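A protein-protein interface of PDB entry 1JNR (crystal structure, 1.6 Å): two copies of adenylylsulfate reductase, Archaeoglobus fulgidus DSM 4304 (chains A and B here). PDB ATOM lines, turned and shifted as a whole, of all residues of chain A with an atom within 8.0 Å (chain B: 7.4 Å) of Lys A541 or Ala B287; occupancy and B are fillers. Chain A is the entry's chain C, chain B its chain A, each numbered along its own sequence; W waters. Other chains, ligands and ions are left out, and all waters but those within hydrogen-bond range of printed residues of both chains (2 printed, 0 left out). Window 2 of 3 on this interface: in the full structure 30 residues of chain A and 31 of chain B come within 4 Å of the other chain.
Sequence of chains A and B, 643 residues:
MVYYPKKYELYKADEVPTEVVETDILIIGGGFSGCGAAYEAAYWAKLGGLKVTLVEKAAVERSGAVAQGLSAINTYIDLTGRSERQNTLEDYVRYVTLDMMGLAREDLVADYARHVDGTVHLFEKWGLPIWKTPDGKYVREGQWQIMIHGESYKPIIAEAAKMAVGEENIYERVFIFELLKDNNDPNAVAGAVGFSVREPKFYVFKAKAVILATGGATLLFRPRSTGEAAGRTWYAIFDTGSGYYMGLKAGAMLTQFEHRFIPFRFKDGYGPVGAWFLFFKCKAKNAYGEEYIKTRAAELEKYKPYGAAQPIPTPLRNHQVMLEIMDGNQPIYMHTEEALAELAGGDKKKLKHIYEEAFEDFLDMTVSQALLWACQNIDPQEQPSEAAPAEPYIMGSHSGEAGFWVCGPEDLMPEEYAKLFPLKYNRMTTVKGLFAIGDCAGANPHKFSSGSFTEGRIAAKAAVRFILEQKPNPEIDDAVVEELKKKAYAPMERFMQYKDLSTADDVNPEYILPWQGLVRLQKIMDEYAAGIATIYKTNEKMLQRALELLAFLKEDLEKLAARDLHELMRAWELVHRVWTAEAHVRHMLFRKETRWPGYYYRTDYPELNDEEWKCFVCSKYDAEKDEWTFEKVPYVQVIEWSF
The side-chain amide nitrogen (ND2) of Asn A539 sits at hydrogen-bond distance from the backbone carbonyl oxygen (O) of Gln B330 (3.0 Å).
O of Gln B330 sits close to SD of Met A542 (3.5 Å).
O of Gly B328 lies within hydrogen-bond range of ND2 of Asn A539 (2.9 Å).
N of Pro B331 lies close to SD of Met A542.
The backbone NH of Met A542 lies within hydrogen-bond range of the side-chain amide oxygen of Asn A539.
The backbone NH (N) of Ala B287 lies within hydrogen-bond range of the backbone carbonyl oxygen (O) of Asn B329 (2.9 Å).
The backbone NH (N) of Glu A540 is in hydrogen-bond range of the side-chain carboxylate (OD2) of Asp A604, 3.0 Å away.
The side-chain amide oxygen (OE1) of Gln A544 lies close to the side-chain amino group (NZ) of Lys A541, at 3.0 Å.
The side-chain amide oxygen (OD1) of Asn A539 sits at hydrogen-bond distance from the backbone NH (N) of Lys A541, 2.9 Å away.
O of Pro B331 sits at hydrogen-bond distance from N of Ala B287 (2.9 Å).
Among the printed residues, pairs that only touch across the chains: Asn A539 with Tyr B288 (3.8 Å), Lys A541 with Ala B287 (3.7 Å), Lys A541 with Pro B331 (3.7 Å) and Asp A604 with Tyr B288 (3.6 Å).
Printed residues of chain B within 4 Å of Met A542: Gln B330 (3.4 Å) and Pro B331 (3.2 Å).
Of the printed residues of chain A, Tyr B288 touches Asn A539 and Asp A604.
Of the printed residues of chain A, Pro B331 touches Lys A541 (3.7 Å) and Met A542 (3.2 Å).
Ile B332 touches none of the printed residues of chain A.
Asn B329 touches none of the printed residues of chain A.
The nearest residue of chain B that does not touch Lys A541 is Gln B330 (4.3 Å).
The nearest printed residue of chain A that does not touch Tyr B288 is Lys A541 (4.8 Å).
Of the 15 printed residues of chain B, 5 touch a printed residue of chain A.
Hydrophobic or aromatic side chains of chain B within 4 Å of the printed part of chain A: Ala B287, Tyr B288 and Pro B331.
Along chain B the printed residues that touch a printed residue of chain A span positions 287 to 331.
Hydrophobic or aromatic side chains of chain A within 4 Å of the printed part of chain B: Met A542.
Along chain A the printed residues that touch a printed residue of chain B span positions 539 to 604.
Among the printed residues, 8 pairs touch across the chains.
No position is printed for both chains.
Water W2 lies within hydrogen-bond range of OH of Tyr B288 (2.9 Å), N of Lys A541 (3.1 Å), OD1 of Asn A539 (3.2 Å) and N of Glu A540 (3.3 Å).
Water W1 bridges O of Gly B328 and O of Thr A538.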
ATOM      1  N   TYR A 528      11.987  15.226   1.147  1.00  0.00           N
ATOM      2  CA  TYR A 528      12.988  14.708   0.223  1.00  0.00           C
ATOM      3  C   TYR A 528      13.115  13.201   0.094  1.00  0.00           C
ATOM      4  O   TYR A 528      13.689  12.717  -0.884  1.00  0.00           O
ATOM      5  CB  TYR A 528      14.374  15.250   0.588  1.00  0.00           C
ATOM      6  CG  TYR A 528      14.471  16.753   0.574  1.00  0.00           C
ATOM      7  CD1 TYR A 528      14.203  17.501   1.721  1.00  0.00           C
ATOM      8  CD2 TYR A 528      14.799  17.432  -0.596  1.00  0.00           C
ATOM      9  CE1 TYR A 528      14.257  18.893   1.698  1.00  0.00           C
ATOM     10  CE2 TYR A 528      14.854  18.818  -0.632  1.00  0.00           C
ATOM     11  CZ  TYR A 528      14.584  19.540   0.516  1.00  0.00           C
ATOM     12  OH  TYR A 528      14.641  20.910   0.472  1.00  0.00           O
ATOM     13  N   THR A 538      10.271  10.559  -5.125  1.00  0.00           N
ATOM     14  CA  THR A 538      11.576  11.163  -4.896  1.00  0.00           C
ATOM     15  C   THR A 538      12.464  10.894  -6.104  1.00  0.00           C
ATOM     16  O   THR A 538      12.045  10.219  -7.049  1.00  0.00           O
ATOM     17  CB  THR A 538      12.253  10.613  -3.616  1.00  0.00           C
ATOM     18  OG1 THR A 538      13.446  11.362  -3.348  1.00  0.00           O
ATOM     19  CG2 THR A 538      12.615   9.149  -3.785  1.00  0.00           C
ATOM     20  N   ASN A 539      13.670  11.450  -6.094  1.00  0.00           N
ATOM     21  CA  ASN A 539      14.615  11.233  -7.186  1.00  0.00           C
ATOM     22  C   ASN A 539      16.024  11.414  -6.640  1.00  0.00           C
ATOM     23  O   ASN A 539      16.199  11.683  -5.451  1.00  0.00           O
ATOM     24  CB  ASN A 539      14.350  12.207  -8.344  1.00  0.00           C
ATOM     25  CG  ASN A 539      14.481  13.662  -7.936  1.00  0.00           C
ATOM     26  OD1 ASN A 539      15.373  14.023  -7.174  1.00  0.00           O
ATOM     27  ND2 ASN A 539      13.600  14.509  -8.462  1.00  0.00           N
ATOM     28  N   GLU A 540      17.026  11.268  -7.499  1.00  0.00           N
ATOM     29  CA  GLU A 540      18.414  11.409  -7.072  1.00  0.00           C
ATOM     30  C   GLU A 540      18.711  12.755  -6.409  1.00  0.00           C
ATOM     31  O   GLU A 540      19.316  12.803  -5.336  1.00  0.00           O
ATOM     32  CB  GLU A 540      19.356  11.215  -8.262  1.00  0.00           C
ATOM     33  CG  GLU A 540      20.827  11.280  -7.876  1.00  0.00           C
ATOM     34  CD  GLU A 540      21.746  11.317  -9.079  1.00  0.00           C
ATOM     35  OE1 GLU A 540      21.669  12.291  -9.855  1.00  0.00           O
ATOM     36  OE2 GLU A 540      22.544  10.370  -9.246  1.00  0.00           O
ATOM     37  N   LYS A 541      18.283  13.842  -7.044  1.00  0.00           N
ATOM     38  CA  LYS A 541      18.523  15.183  -6.526  1.00  0.00           C
ATOM     39  C   LYS A 541      17.925  15.391  -5.140  1.00  0.00           C
ATOM     40  O   LYS A 541      18.592  15.908  -4.237  1.00  0.00           O
ATOM     41  CB  LYS A 541      17.958  16.220  -7.498  1.00  0.00           C
ATOM     42  CG  LYS A 541      18.525  16.141  -8.915  1.00  0.00           C
ATOM     43  CD  LYS A 541      19.877  16.813  -9.031  1.00  0.00           C
ATOM     44  CE  LYS A 541      20.922  16.134  -8.170  1.00  0.00           C
ATOM     45  NZ  LYS A 541      22.229  16.864  -8.170  1.00  0.00           N
ATOM     46  N   MET A 542      16.662  15.004  -4.967  1.00  0.00           N
ATOM     47  CA  MET A 542      16.003  15.159  -3.672  1.00  0.00           C
ATOM     48  C   MET A 542      16.697  14.316  -2.610  1.00  0.00           C
ATOM     49  O   MET A 542      16.913  14.773  -1.489  1.00  0.00           O
ATOM     50  CB  MET A 542      14.528  14.757  -3.770  1.00  0.00           C
ATOM     51  CG  MET A 542      13.701  15.672  -4.657  1.00  0.00           C
ATOM     52  SD  MET A 542      13.716  17.381  -4.077  1.00  0.00           S
ATOM     53  CE  MET A 542      12.276  17.390  -3.017  1.00  0.00           C
ATOM     54  N   LEU A 543      17.052  13.084  -2.958  1.00  0.00           N
ATOM     55  CA  LEU A 543      17.733  12.217  -1.999  1.00  0.00           C
ATOM     56  C   LEU A 543      19.103  12.786  -1.619  1.00  0.00           C
ATOM     57  O   LEU A 543      19.501  12.735  -0.456  1.00  0.00           O
ATOM     58  CB  LEU A 543      17.873  10.807  -2.575  1.00  0.00           C
ATOM     59  CG  LEU A 543      16.539  10.070  -2.717  1.00  0.00           C
ATOM     60  CD1 LEU A 543      16.744   8.780  -3.487  1.00  0.00           C
ATOM     61  CD2 LEU A 543      15.954   9.791  -1.334  1.00  0.00           C
ATOM     62  N   GLN A 544      19.822  13.337  -2.593  1.00  0.00           N
ATOM     63  CA  GLN A 544      21.129  13.921  -2.307  1.00  0.00           C
ATOM     64  C   GLN A 544      20.969  15.122  -1.378  1.00  0.00           C
ATOM     65  O   GLN A 544      21.765  15.312  -0.457  1.00  0.00           O
ATOM     66  CB  GLN A 544      21.828  14.337  -3.606  1.00  0.00           C
ATOM     67  CG  GLN A 544      22.206  13.157  -4.490  1.00  0.00           C
ATOM     68  CD  GLN A 544      22.953  13.568  -5.744  1.00  0.00           C
ATOM     69  OE1 GLN A 544      22.515  14.451  -6.480  1.00  0.00           O
ATOM     70  NE2 GLN A 544      24.085  12.920  -5.998  1.00  0.00           N
ATOM     71  N   ARG A 545      19.939  15.933  -1.608  1.00  0.00           N
ATOM     72  CA  ARG A 545      19.715  17.082  -0.739  1.00  0.00           C
ATOM     73  C   ARG A 545      19.364  16.580   0.657  1.00  0.00           C
ATOM     74  O   ARG A 545      19.754  17.181   1.655  1.00  0.00           O
ATOM     75  CB  ARG A 545      18.587  17.968  -1.275  1.00  0.00           C
ATOM     76  CG  ARG A 545      18.303  19.192  -0.403  1.00  0.00           C
ATOM     77  CD  ARG A 545      19.579  19.969  -0.091  1.00  0.00           C
ATOM     78  NE  ARG A 545      19.300  21.260   0.532  1.00  0.00           N
ATOM     79  CZ  ARG A 545      20.220  22.026   1.111  1.00  0.00           C
ATOM     80  NH1 ARG A 545      21.486  21.633   1.157  1.00  0.00           N
ATOM     81  NH2 ARG A 545      19.875  23.193   1.637  1.00  0.00           N
ATOM     82  N   ALA A 546      18.628  15.472   0.727  1.00  0.00           N
ATOM     83  CA  ALA A 546      18.264  14.908   2.020  1.00  0.00           C
ATOM     84  C   ALA A 546      19.539  14.595   2.797  1.00  0.00           C
ATOM     85  O   ALA A 546      19.633  14.883   3.989  1.00  0.00           O
ATOM     86  CB  ALA A 546      17.437  13.635   1.835  1.00  0.00           C
ATOM     87  N   LEU A 547      20.527  14.011   2.122  1.00  0.00           N
ATOM     88  CA  LEU A 547      21.786  13.678   2.787  1.00  0.00           C
ATOM     89  C   LEU A 547      22.488  14.934   3.297  1.00  0.00           C
ATOM     90  O   LEU A 547      23.066  14.931   4.383  1.00  0.00           O
ATOM     91  CB  LEU A 547      22.711  12.895   1.842  1.00  0.00           C
ATOM     92  CG  LEU A 547      22.212  11.500   1.444  1.00  0.00           C
ATOM     93  CD1 LEU A 547      23.222  10.832   0.521  1.00  0.00           C
ATOM     94  CD2 LEU A 547      21.996  10.648   2.690  1.00  0.00           C
ATOM     95  N   GLU A 548      22.430  16.013   2.522  1.00  0.00           N
ATOM     96  CA  GLU A 548      23.057  17.260   2.937  1.00  0.00           C
ATOM     97  C   GLU A 548      22.383  17.804   4.191  1.00  0.00           C
ATOM     98  O   GLU A 548      23.050  18.239   5.130  1.00  0.00           O
ATOM     99  CB  GLU A 548      22.974  18.295   1.812  1.00  0.00           C
ATOM    100  CG  GLU A 548      23.955  18.043   0.681  1.00  0.00           C
ATOM    101  CD  GLU A 548      23.663  18.884  -0.546  1.00  0.00           C
ATOM    102  OE1 GLU A 548      23.051  19.961  -0.400  1.00  0.00           O
ATOM    103  OE2 GLU A 548      24.057  18.469  -1.658  1.00  0.00           O
ATOM    104  N   LEU A 589      18.700   5.802  -2.654  1.00  0.00           N
ATOM    105  CA  LEU A 589      19.537   6.450  -3.657  1.00  0.00           C
ATOM    106  C   LEU A 589      20.315   5.421  -4.477  1.00  0.00           C
ATOM    107  O   LEU A 589      20.481   5.573  -5.693  1.00  0.00           O
ATOM    108  CB  LEU A 589      20.508   7.416  -2.973  1.00  0.00           C
ATOM    109  CG  LEU A 589      21.528   8.146  -3.852  1.00  0.00           C
ATOM    110  CD1 LEU A 589      20.819   8.912  -4.964  1.00  0.00           C
ATOM    111  CD2 LEU A 589      22.343   9.096  -2.985  1.00  0.00           C
ATOM    112  N   ARG A 602      10.677   6.335  -7.675  1.00  0.00           N
ATOM    113  CA  ARG A 602      11.842   7.122  -8.044  1.00  0.00           C
ATOM    114  C   ARG A 602      11.432   7.628  -9.416  1.00  0.00           C
ATOM    115  O   ARG A 602      11.387   6.870 -10.383  1.00  0.00           O
ATOM    116  CB  ARG A 602      13.107   6.272  -8.125  1.00  0.00           C
ATOM    117  CG  ARG A 602      13.758   6.090  -6.766  1.00  0.00           C
ATOM    118  CD  ARG A 602      15.230   5.786  -6.868  1.00  0.00           C
ATOM    119  NE  ARG A 602      15.978   6.838  -7.558  1.00  0.00           N
ATOM    120  CZ  ARG A 602      17.304   6.917  -7.552  1.00  0.00           C
ATOM    121  NH1 ARG A 602      18.012   6.015  -6.884  1.00  0.00           N
ATOM    122  NH2 ARG A 602      17.926   7.866  -8.235  1.00  0.00           N
ATOM    123  N   ASP A 604      12.965   9.339 -11.447  1.00  0.00           N
ATOM    124  CA  ASP A 604      14.049   9.314 -12.427  1.00  0.00           C
ATOM    125  C   ASP A 604      14.332   7.897 -12.934  1.00  0.00           C
ATOM    126  O   ASP A 604      15.026   7.715 -13.932  1.00  0.00           O
ATOM    127  CB  ASP A 604      15.322   9.975 -11.862  1.00  0.00           C
ATOM    128  CG  ASP A 604      15.717   9.458 -10.486  1.00  0.00           C
ATOM    129  OD1 ASP A 604      14.902   8.793  -9.816  1.00  0.00           O
ATOM    130  OD2 ASP A 604      16.861   9.746 -10.070  1.00  0.00           O
ATOM    131  N   LYS B 285      14.778  27.074 -12.387  1.00  0.00           N
ATOM    132  CA  LYS B 285      14.907  25.831 -13.141  1.00  0.00           C
ATOM    133  C   LYS B 285      14.621  24.643 -12.247  1.00  0.00           C
ATOM    134  O   LYS B 285      14.779  24.727 -11.031  1.00  0.00           O
ATOM    135  CB  LYS B 285      16.314  25.689 -13.710  1.00  0.00           C
ATOM    136  CG  LYS B 285      16.754  26.851 -14.602  1.00  0.00           C
ATOM    137  CD  LYS B 285      18.214  26.700 -15.021  1.00  0.00           C
ATOM    138  CE  LYS B 285      18.670  27.870 -15.884  1.00  0.00           C
ATOM    139  NZ  LYS B 285      20.125  27.775 -16.198  1.00  0.00           N
ATOM    140  N   ASN B 286      14.199  23.536 -12.846  1.00  0.00           N
ATOM    141  CA  ASN B 286      13.921  22.351 -12.057  1.00  0.00           C
ATOM    142  C   ASN B 286      15.224  21.637 -11.733  1.00  0.00           C
ATOM    143  O   ASN B 286      16.308  22.116 -12.070  1.00  0.00           O
ATOM    144  CB  ASN B 286      12.945  21.410 -12.779  1.00  0.00           C
ATOM    145  CG  ASN B 286      13.485  20.880 -14.093  1.00  0.00           C
ATOM    146  OD1 ASN B 286      14.692  20.860 -14.326  1.00  0.00           O
ATOM    147  ND2 ASN B 286      12.581  20.424 -14.955  1.00  0.00           N
ATOM    148  N   ALA B 287      15.112  20.491 -11.073  1.00  0.00           N
ATOM    149  CA  ALA B 287      16.275  19.715 -10.662  1.00  0.00           C
ATOM    150  C   ALA B 287      17.222  19.332 -11.792  1.00  0.00           C
ATOM    151  O   ALA B 287      18.402  19.080 -11.553  1.00  0.00           O
ATOM    152  CB  ALA B 287      15.816  18.458  -9.935  1.00  0.00           C
ATOM    153  N   TYR B 288      16.707  19.294 -13.016  1.00  0.00           N
ATOM    154  CA  TYR B 288      17.523  18.906 -14.156  1.00  0.00           C
ATOM    155  C   TYR B 288      18.062  20.067 -14.976  1.00  0.00           C
ATOM    156  O   TYR B 288      18.648  19.864 -16.038  1.00  0.00           O
ATOM    157  CB  TYR B 288      16.728  17.947 -15.038  1.00  0.00           C
ATOM    158  CG  TYR B 288      16.222  16.764 -14.250  1.00  0.00           C
ATOM    159  CD1 TYR B 288      14.888  16.683 -13.848  1.00  0.00           C
ATOM    160  CD2 TYR B 288      17.098  15.759 -13.842  1.00  0.00           C
ATOM    161  CE1 TYR B 288      14.441  15.626 -13.053  1.00  0.00           C
ATOM    162  CE2 TYR B 288      16.664  14.704 -13.049  1.00  0.00           C
ATOM    163  CZ  TYR B 288      15.338  14.643 -12.657  1.00  0.00           C
ATOM    164  OH  TYR B 288      14.923  13.603 -11.855  1.00  0.00           O
ATOM    165  N   GLY B 289      17.860  21.282 -14.479  1.00  0.00           N
ATOM    166  CA  GLY B 289      18.360  22.453 -15.176  1.00  0.00           C
ATOM    167  C   GLY B 289      17.452  23.020 -16.250  1.00  0.00           C
ATOM    168  O   GLY B 289      17.880  23.864 -17.036  1.00  0.00           O
ATOM    169  N   GLU B 290      16.202  22.569 -16.290  1.00  0.00           N
ATOM    170  CA  GLU B 290      15.258  23.070 -17.283  1.00  0.00           C
ATOM    171  C   GLU B 290      14.524  24.303 -16.776  1.00  0.00           C
ATOM    172  O   GLU B 290      14.023  24.311 -15.649  1.00  0.00           O
ATOM    173  CB  GLU B 290      14.207  22.014 -17.621  1.00  0.00           C
ATOM    174  CG  GLU B 290      14.724  20.758 -18.280  1.00  0.00           C
ATOM    175  CD  GLU B 290      13.594  19.817 -18.648  1.00  0.00           C
ATOM    176  OE1 GLU B 290      12.841  19.404 -17.740  1.00  0.00           O
ATOM    177  OE2 GLU B 290      13.454  19.494 -19.845  1.00  0.00           O
ATOM    178  N   TYR B 292      11.492  25.817 -16.674  1.00  0.00           N
ATOM    179  CA  TYR B 292      10.116  25.419 -16.935  1.00  0.00           C
ATOM    180  C   TYR B 292       9.143  26.448 -17.496  1.00  0.00           C
ATOM    181  O   TYR B 292       8.083  26.069 -17.991  1.00  0.00           O
ATOM    182  CB  TYR B 292       9.522  24.748 -15.688  1.00  0.00           C
ATOM    183  CG  TYR B 292       9.563  25.587 -14.437  1.00  0.00           C
ATOM    184  CD1 TYR B 292       8.579  26.538 -14.178  1.00  0.00           C
ATOM    185  CD2 TYR B 292      10.600  25.438 -13.514  1.00  0.00           C
ATOM    186  CE1 TYR B 292       8.623  27.321 -13.032  1.00  0.00           C
ATOM    187  CE2 TYR B 292      10.654  26.216 -12.367  1.00  0.00           C
ATOM    188  CZ  TYR B 292       9.665  27.153 -12.132  1.00  0.00           C
ATOM    189  OH  TYR B 292       9.714  27.924 -10.996  1.00  0.00           O
ATOM    190  N   GLU B 324       5.634  20.669 -12.687  1.00  0.00           N
ATOM    191  CA  GLU B 324       6.991  20.208 -12.418  1.00  0.00           C
ATOM    192  C   GLU B 324       7.017  19.413 -11.121  1.00  0.00           C
ATOM    193  O   GLU B 324       7.685  18.382 -11.024  1.00  0.00           O
ATOM    194  CB  GLU B 324       7.943  21.398 -12.304  1.00  0.00           C
ATOM    195  CG  GLU B 324       8.246  22.067 -13.627  1.00  0.00           C
ATOM    196  CD  GLU B 324       8.989  21.146 -14.567  1.00  0.00           C
ATOM    197  OE1 GLU B 324       9.995  20.549 -14.131  1.00  0.00           O
ATOM    198  OE2 GLU B 324       8.572  21.017 -15.737  1.00  0.00           O
ATOM    199  N   GLY B 328       7.615  15.250 -10.421  1.00  0.00           N
ATOM    200  CA  GLY B 328       8.732  14.891  -9.565  1.00  0.00           C
ATOM    201  C   GLY B 328      10.047  15.519  -9.992  1.00  0.00           C
ATOM    202  O   GLY B 328      11.102  14.897  -9.870  1.00  0.00           O
ATOM    203  N   ASN B 329       9.996  16.756 -10.477  1.00  0.00           N
ATOM    204  CA  ASN B 329      11.202  17.436 -10.934  1.00  0.00           C
ATOM    205  C   ASN B 329      11.820  18.398  -9.932  1.00  0.00           C
ATOM    206  O   ASN B 329      12.570  19.302 -10.303  1.00  0.00           O
ATOM    207  CB  ASN B 329      10.932  18.162 -12.250  1.00  0.00           C
ATOM    208  CG  ASN B 329      10.621  17.203 -13.378  1.00  0.00           C
ATOM    209  OD1 ASN B 329      10.988  16.029 -13.318  1.00  0.00           O
ATOM    210  ND2 ASN B 329       9.958  17.695 -14.417  1.00  0.00           N
ATOM    211  N   GLN B 330      11.498  18.208  -8.660  1.00  0.00           N
ATOM    212  CA  GLN B 330      12.074  19.041  -7.615  1.00  0.00           C
ATOM    213  C   GLN B 330      13.465  18.497  -7.308  1.00  0.00           C
ATOM    214  O   GLN B 330      13.769  17.342  -7.601  1.00  0.00           O
ATOM    215  CB  GLN B 330      11.195  19.010  -6.364  1.00  0.00           C
ATOM    216  CG  GLN B 330       9.950  19.866  -6.500  1.00  0.00           C
ATOM    217  CD  GLN B 330       9.135  19.931  -5.225  1.00  0.00           C
ATOM    218  OE1 GLN B 330       8.495  18.954  -4.827  1.00  0.00           O
ATOM    219  NE2 GLN B 330       9.157  21.086  -4.571  1.00  0.00           N
ATOM    220  N   PRO B 331      14.326  19.314  -6.690  1.00  0.00           N
ATOM    221  CA  PRO B 331      14.086  20.696  -6.266  1.00  0.00           C
ATOM    222  C   PRO B 331      13.994  21.706  -7.401  1.00  0.00           C
ATOM    223  O   PRO B 331      14.580  21.515  -8.467  1.00  0.00           O
ATOM    224  CB  PRO B 331      15.292  21.004  -5.368  1.00  0.00           C
ATOM    225  CG  PRO B 331      15.848  19.646  -5.002  1.00  0.00           C
ATOM    226  CD  PRO B 331      15.667  18.874  -6.274  1.00  0.00           C
ATOM    227  N   ILE B 332      13.243  22.773  -7.160  1.00  0.00           N
ATOM    228  CA  ILE B 332      13.129  23.859  -8.117  1.00  0.00           C
ATOM    229  C   ILE B 332      14.101  24.889  -7.562  1.00  0.00           C
ATOM    230  O   ILE B 332      14.041  25.226  -6.379  1.00  0.00           O
ATOM    231  CB  ILE B 332      11.709  24.455  -8.145  1.00  0.00           C
ATOM    232  CG1 ILE B 332      10.724  23.425  -8.705  1.00  0.00           C
ATOM    233  CG2 ILE B 332      11.699  25.726  -8.982  1.00  0.00           C
ATOM    234  CD1 ILE B 332       9.307  23.940  -8.844  1.00  0.00           C
ATOM    235  N   TYR B 333      14.995  25.381  -8.413  1.00  0.00           N
ATOM    236  CA  TYR B 333      16.008  26.337  -7.981  1.00  0.00           C
ATOM    237  C   TYR B 333      15.942  27.735  -8.554  1.00  0.00           C
ATOM    238  O   TYR B 333      15.649  27.922  -9.733  1.00  0.00           O
ATOM    239  CB  TYR B 333      17.410  25.817  -8.309  1.00  0.00           C
ATOM    240  CG  TYR B 333      17.855  24.636  -7.503  1.00  0.00           C
ATOM    241  CD1 TYR B 333      17.720  23.339  -7.995  1.00  0.00           C
ATOM    242  CD2 TYR B 333      18.415  24.812  -6.241  1.00  0.00           C
ATOM    243  CE1 TYR B 333      18.135  22.247  -7.243  1.00  0.00           C
ATOM    244  CE2 TYR B 333      18.829  23.734  -5.486  1.00  0.00           C
ATOM    245  CZ  TYR B 333      18.687  22.455  -5.990  1.00  0.00           C
ATOM    246  OH  TYR B 333      19.100  21.391  -5.227  1.00  0.00           O
ATOM    247  N   HIS B 335      18.302  30.354  -9.538  1.00  0.00           N
ATOM    248  CA  HIS B 335      19.738  30.433  -9.795  1.00  0.00           C
ATOM    249  C   HIS B 335      20.352  31.813  -9.625  1.00  0.00           C
ATOM    250  O   HIS B 335      20.782  32.457 -10.582  1.00  0.00           O
ATOM    251  CB  HIS B 335      20.040  29.861 -11.180  1.00  0.00           C
ATOM    252  CG  HIS B 335      20.011  28.365 -11.216  1.00  0.00           C
ATOM    253  ND1 HIS B 335      21.094  27.593 -10.856  1.00  0.00           N
ATOM    254  CD2 HIS B 335      19.003  27.499 -11.480  1.00  0.00           C
ATOM    255  CE1 HIS B 335      20.755  26.317 -10.894  1.00  0.00           C
ATOM    256  NE2 HIS B 335      19.490  26.233 -11.269  1.00  0.00           N
HETATM  257  O   HOH W   1      10.563  13.081  -7.353  1.00  0.00           O
HETATM  258  O   HOH W   2      17.011  13.534  -9.843  1.00  0.00           O
